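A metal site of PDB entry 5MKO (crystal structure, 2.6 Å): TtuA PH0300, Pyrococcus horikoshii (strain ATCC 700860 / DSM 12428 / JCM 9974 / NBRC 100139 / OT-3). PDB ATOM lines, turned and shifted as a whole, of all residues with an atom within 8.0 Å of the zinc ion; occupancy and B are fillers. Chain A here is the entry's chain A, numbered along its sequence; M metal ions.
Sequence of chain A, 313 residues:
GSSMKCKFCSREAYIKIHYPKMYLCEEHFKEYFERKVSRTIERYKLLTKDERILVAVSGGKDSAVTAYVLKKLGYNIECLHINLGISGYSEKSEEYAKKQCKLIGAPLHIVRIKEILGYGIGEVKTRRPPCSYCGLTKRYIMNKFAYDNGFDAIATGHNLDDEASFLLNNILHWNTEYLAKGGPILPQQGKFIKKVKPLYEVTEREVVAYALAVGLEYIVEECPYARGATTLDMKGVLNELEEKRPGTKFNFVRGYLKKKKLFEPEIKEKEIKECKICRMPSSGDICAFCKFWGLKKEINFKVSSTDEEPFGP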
ATOM      1  N   LYS A   5     -16.102  18.686   9.775  1.00  0.00           N
ATOM      2  CA  LYS A   5     -15.135  18.797  10.881  1.00  0.00           C
ATOM      3  C   LYS A   5     -14.842  17.413  11.472  1.00  0.00           C
ATOM      4  O   LYS A   5     -15.536  16.446  11.126  1.00  0.00           O
ATOM      5  CB  LYS A   5     -15.630  19.777  11.962  1.00  0.00           C
ATOM      6  CG  LYS A   5     -15.673  21.245  11.530  1.00  0.00           C
ATOM      7  CD  LYS A   5     -14.312  21.937  11.598  1.00  0.00           C
ATOM      8  CE  LYS A   5     -14.341  23.314  10.970  1.00  0.00           C
ATOM      9  NZ  LYS A   5     -13.012  23.962  11.004  1.00  0.00           N
ATOM     10  N   CYS A   6     -13.818  17.317  12.347  1.00  0.00           N
ATOM     11  CA  CYS A   6     -13.434  16.055  13.003  1.00  0.00           C
ATOM     12  C   CYS A   6     -14.539  15.546  13.939  1.00  0.00           C
ATOM     13  O   CYS A   6     -15.143  16.330  14.673  1.00  0.00           O
ATOM     14  CB  CYS A   6     -12.100  16.213  13.743  1.00  0.00           C
ATOM     15  SG  CYS A   6     -11.521  14.690  14.543  1.00  0.00           S
ATOM     16  N   LYS A   7     -14.768  14.222  13.923  1.00  0.00           N
ATOM     17  CA  LYS A   7     -15.757  13.516  14.748  1.00  0.00           C
ATOM     18  C   LYS A   7     -15.378  13.531  16.246  1.00  0.00           C
ATOM     19  O   LYS A   7     -16.221  13.227  17.096  1.00  0.00           O
ATOM     20  CB  LYS A   7     -15.922  12.067  14.254  1.00  0.00           C
ATOM     21  CG  LYS A   7     -17.281  11.453  14.514  1.00  0.00           C
ATOM     22  CD  LYS A   7     -17.349  10.010  14.040  1.00  0.00           C
ATOM     23  CE  LYS A   7     -18.768   9.518  13.894  1.00  0.00           C
ATOM     24  NZ  LYS A   7     -18.825   8.203  13.204  1.00  0.00           N
ATOM     25  N   PHE A   8     -14.112  13.874  16.550  1.00  0.00           N
ATOM     26  CA  PHE A   8     -13.564  13.895  17.898  1.00  0.00           C
ATOM     27  C   PHE A   8     -13.140  15.278  18.381  1.00  0.00           C
ATOM     28  O   PHE A   8     -13.146  15.499  19.589  1.00  0.00           O
ATOM     29  CB  PHE A   8     -12.405  12.885  18.027  1.00  0.00           C
ATOM     30  CG  PHE A   8     -12.854  11.442  17.953  1.00  0.00           C
ATOM     31  CD1 PHE A   8     -13.134  10.837  16.730  1.00  0.00           C
ATOM     32  CD2 PHE A   8     -12.972  10.678  19.113  1.00  0.00           C
ATOM     33  CE1 PHE A   8     -13.558   9.512  16.667  1.00  0.00           C
ATOM     34  CE2 PHE A   8     -13.384   9.338  19.047  1.00  0.00           C
ATOM     35  CZ  PHE A   8     -13.671   8.765  17.827  1.00  0.00           C
ATOM     36  N   CYS A   9     -12.768  16.202  17.471  1.00  0.00           N
ATOM     37  CA  CYS A   9     -12.367  17.551  17.905  1.00  0.00           C
ATOM     38  C   CYS A   9     -12.874  18.679  16.988  1.00  0.00           C
ATOM     39  O   CYS A   9     -13.544  18.423  15.974  1.00  0.00           O
ATOM     40  CB  CYS A   9     -10.864  17.641  18.147  1.00  0.00           C
ATOM     41  SG  CYS A   9      -9.853  17.689  16.649  1.00  0.00           S
ATOM     42  N   SER A  10     -12.581  19.941  17.384  1.00  0.00           N
ATOM     43  CA  SER A  10     -12.969  21.180  16.698  1.00  0.00           C
ATOM     44  C   SER A  10     -11.904  21.625  15.670  1.00  0.00           C
ATOM     45  O   SER A  10     -11.505  22.796  15.634  1.00  0.00           O
ATOM     46  CB  SER A  10     -13.250  22.272  17.723  1.00  0.00           C
ATOM     47  OG  SER A  10     -13.680  23.457  17.083  1.00  0.00           O
ATOM     48  N   ARG A  11     -11.471  20.677  14.839  1.00  0.00           N
ATOM     49  CA  ARG A  11     -10.488  20.913  13.775  1.00  0.00           C
ATOM     50  C   ARG A  11     -11.063  20.447  12.444  1.00  0.00           C
ATOM     51  O   ARG A  11     -11.902  19.524  12.412  1.00  0.00           O
ATOM     52  CB  ARG A  11      -9.164  20.182  14.047  1.00  0.00           C
ATOM     53  CG  ARG A  11      -8.332  20.743  15.191  1.00  0.00           C
ATOM     54  CD  ARG A  11      -7.072  19.913  15.388  1.00  0.00           C
ATOM     55  NE  ARG A  11      -6.328  20.306  16.586  1.00  0.00           N
ATOM     56  CZ  ARG A  11      -6.313  19.623  17.729  1.00  0.00           C
ATOM     57  NH1 ARG A  11      -7.018  18.507  17.848  1.00  0.00           N
ATOM     58  NH2 ARG A  11      -5.599  20.065  18.755  1.00  0.00           N
ATOM     59  N   GLU A  12     -10.610  21.072  11.349  1.00  0.00           N
ATOM     60  CA  GLU A  12     -11.021  20.738   9.987  1.00  0.00           C
ATOM     61  C   GLU A  12     -10.568  19.310   9.665  1.00  0.00           C
ATOM     62  O   GLU A  12      -9.427  18.942   9.971  1.00  0.00           O
ATOM     63  CB  GLU A  12     -10.439  21.751   8.990  1.00  0.00           C
ATOM     64  CG  GLU A  12     -11.287  21.890   7.731  1.00  0.00           C
ATOM     65  CD  GLU A  12     -10.709  22.755   6.625  1.00  0.00           C
ATOM     66  OE1 GLU A  12     -10.896  22.393   5.439  1.00  0.00           O
ATOM     67  OE2 GLU A  12     -10.084  23.804   6.931  1.00  0.00           O
ATOM     68  N   ALA A  13     -11.486  18.506   9.108  1.00  0.00           N
ATOM     69  CA  ALA A  13     -11.238  17.104   8.750  1.00  0.00           C
ATOM     70  C   ALA A  13     -10.163  16.992   7.676  1.00  0.00           C
ATOM     71  O   ALA A  13     -10.219  17.685   6.647  1.00  0.00           O
ATOM     72  CB  ALA A  13     -12.521  16.420   8.296  1.00  0.00           C
ATOM     73  N   TYR A  14      -9.154  16.170   7.958  1.00  0.00           N
ATOM     74  CA  TYR A  14      -8.001  15.910   7.098  1.00  0.00           C
ATOM     75  C   TYR A  14      -8.376  14.835   6.074  1.00  0.00           C
ATOM     76  O   TYR A  14      -8.034  14.971   4.893  1.00  0.00           O
ATOM     77  CB  TYR A  14      -6.816  15.464   7.987  1.00  0.00           C
ATOM     78  CG  TYR A  14      -5.578  15.001   7.257  1.00  0.00           C
ATOM     79  CD1 TYR A  14      -4.773  15.899   6.554  1.00  0.00           C
ATOM     80  CD2 TYR A  14      -5.146  13.681   7.349  1.00  0.00           C
ATOM     81  CE1 TYR A  14      -3.624  15.479   5.907  1.00  0.00           C
ATOM     82  CE2 TYR A  14      -3.991  13.254   6.700  1.00  0.00           C
ATOM     83  CZ  TYR A  14      -3.231  14.159   5.976  1.00  0.00           C
ATOM     84  OH  TYR A  14      -2.095  13.756   5.332  1.00  0.00           O
ATOM     85  N   TYR A  23     -15.282  11.343   9.590  1.00  0.00           N
ATOM     86  CA  TYR A  23     -14.371  12.419   9.248  1.00  0.00           C
ATOM     87  C   TYR A  23     -13.421  12.630  10.421  1.00  0.00           C
ATOM     88  O   TYR A  23     -13.880  12.772  11.554  1.00  0.00           O
ATOM     89  CB  TYR A  23     -15.139  13.724   8.952  1.00  0.00           C
ATOM     90  CG  TYR A  23     -15.805  13.757   7.584  1.00  0.00           C
ATOM     91  CD1 TYR A  23     -17.106  13.284   7.413  1.00  0.00           C
ATOM     92  CD2 TYR A  23     -15.156  14.293   6.480  1.00  0.00           C
ATOM     93  CE1 TYR A  23     -17.723  13.318   6.167  1.00  0.00           C
ATOM     94  CE2 TYR A  23     -15.762  14.335   5.232  1.00  0.00           C
ATOM     95  CZ  TYR A  23     -17.055  13.854   5.074  1.00  0.00           C
ATOM     96  OH  TYR A  23     -17.664  13.879   3.839  1.00  0.00           O
ATOM     97  N   LEU A  24     -12.100  12.617  10.146  1.00  0.00           N
ATOM     98  CA  LEU A  24     -11.077  12.796  11.183  1.00  0.00           C
ATOM     99  C   LEU A  24     -10.037  13.852  10.797  1.00  0.00           C
ATOM    100  O   LEU A  24      -9.737  14.006   9.616  1.00  0.00           O
ATOM    101  CB  LEU A  24     -10.359  11.475  11.493  1.00  0.00           C
ATOM    102  CG  LEU A  24     -11.169  10.334  12.116  1.00  0.00           C
ATOM    103  CD1 LEU A  24     -10.359   9.051  12.134  1.00  0.00           C
ATOM    104  CD2 LEU A  24     -11.605  10.669  13.531  1.00  0.00           C
ATOM    105  N   CYS A  25      -9.471  14.543  11.792  1.00  0.00           N
ATOM    106  CA  CYS A  25      -8.439  15.545  11.590  1.00  0.00           C
ATOM    107  C   CYS A  25      -7.046  14.873  11.503  1.00  0.00           C
ATOM    108  O   CYS A  25      -6.942  13.656  11.670  1.00  0.00           O
ATOM    109  CB  CYS A  25      -8.485  16.631  12.655  1.00  0.00           C
ATOM    110  SG  CYS A  25      -7.603  16.234  14.193  1.00  0.00           S
ATOM    111  N   GLU A  26      -6.007  15.673  11.243  1.00  0.00           N
ATOM    112  CA  GLU A  26      -4.612  15.255  11.109  1.00  0.00           C
ATOM    113  C   GLU A  26      -4.123  14.416  12.308  1.00  0.00           C
ATOM    114  O   GLU A  26      -3.364  13.479  12.120  1.00  0.00           O
ATOM    115  CB  GLU A  26      -3.709  16.488  10.915  1.00  0.00           C
ATOM    116  CG  GLU A  26      -2.410  16.211  10.195  1.00  0.00           C
ATOM    117  CD  GLU A  26      -1.596  17.444   9.844  1.00  0.00           C
ATOM    118  OE1 GLU A  26      -2.128  18.353   9.166  1.00  0.00           O
ATOM    119  OE2 GLU A  26      -0.392  17.484  10.209  1.00  0.00           O
ATOM    120  N   GLU A  27      -4.586  14.769  13.521  1.00  0.00           N
ATOM    121  CA  GLU A  27      -4.203  14.118  14.778  1.00  0.00           C
ATOM    122  C   GLU A  27      -5.030  12.878  15.117  1.00  0.00           C
ATOM    123  O   GLU A  27      -4.452  11.875  15.536  1.00  0.00           O
ATOM    124  CB  GLU A  27      -4.205  15.117  15.945  1.00  0.00           C
ATOM    125  CG  GLU A  27      -3.149  16.212  15.817  1.00  0.00           C
ATOM    126  CD  GLU A  27      -1.725  15.775  15.569  1.00  0.00           C
ATOM    127  OE1 GLU A  27      -1.235  14.854  16.266  1.00  0.00           O
ATOM    128  OE2 GLU A  27      -1.082  16.357  14.662  1.00  0.00           O
ATOM    129  N   HIS A  28      -6.357  12.938  14.929  1.00  0.00           N
ATOM    130  CA  HIS A  28      -7.225  11.801  15.232  1.00  0.00           C
ATOM    131  C   HIS A  28      -7.107  10.686  14.203  1.00  0.00           C
ATOM    132  O   HIS A  28      -7.420   9.538  14.529  1.00  0.00           O
ATOM    133  CB  HIS A  28      -8.678  12.235  15.449  1.00  0.00           C
ATOM    134  CG  HIS A  28      -8.865  12.907  16.774  1.00  0.00           C
ATOM    135  ND1 HIS A  28      -8.873  14.283  16.897  1.00  0.00           N
ATOM    136  CD2 HIS A  28      -8.930  12.362  18.012  1.00  0.00           C
ATOM    137  CE1 HIS A  28      -8.986  14.535  18.182  1.00  0.00           C
ATOM    138  NE2 HIS A  28      -9.026  13.406  18.902  1.00  0.00           N
ATOM    139  N   PHE A  29      -6.597  11.006  13.000  1.00  0.00           N
ATOM    140  CA  PHE A  29      -6.341  10.013  11.957  1.00  0.00           C
ATOM    141  C   PHE A  29      -5.077   9.233  12.308  1.00  0.00           C
ATOM    142  O   PHE A  29      -5.062   8.007  12.165  1.00  0.00           O
ATOM    143  CB  PHE A  29      -6.223  10.678  10.575  1.00  0.00           C
ATOM    144  CG  PHE A  29      -5.590   9.770   9.541  1.00  0.00           C
ATOM    145  CD1 PHE A  29      -6.279   8.672   9.034  1.00  0.00           C
ATOM    146  CD2 PHE A  29      -4.288   9.988   9.113  1.00  0.00           C
ATOM    147  CE1 PHE A  29      -5.684   7.828   8.111  1.00  0.00           C
ATOM    148  CE2 PHE A  29      -3.694   9.144   8.190  1.00  0.00           C
ATOM    149  CZ  PHE A  29      -4.394   8.074   7.694  1.00  0.00           C
HETATM  150 ZN    ZN M   1      -9.749  15.618  15.357  1.00  0.00          ZN
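The side-chain sulfur of Cys 6 sits close to the backbone NH of Phe 8 (3.4 Å).
The backbone NH (N) of Cys 6 sits at hydrogen-bond distance from the backbone carbonyl oxygen (O) of Arg 11 (2.9 Å).
The guanidinium group (NH1) of Arg 11 sits close to the side-chain sulfur (SG) of Cys 9, at 3.2 Å.
The backbone NH of Glu 27 sits close to the side-chain sulfur of Cys 25, at 3.4 Å.
Four residues have an atom within 4 Å of the zinc ion: Cys 6, Cys 9, Cys 25 and His 28.
The zinc ion is bound by SG of Cys 6 (2.2 Å), ND1 of His 28 (2.2 Å), SG of Cys 9 (2.4 Å) and SG of Cys 25 (2.5 Å).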
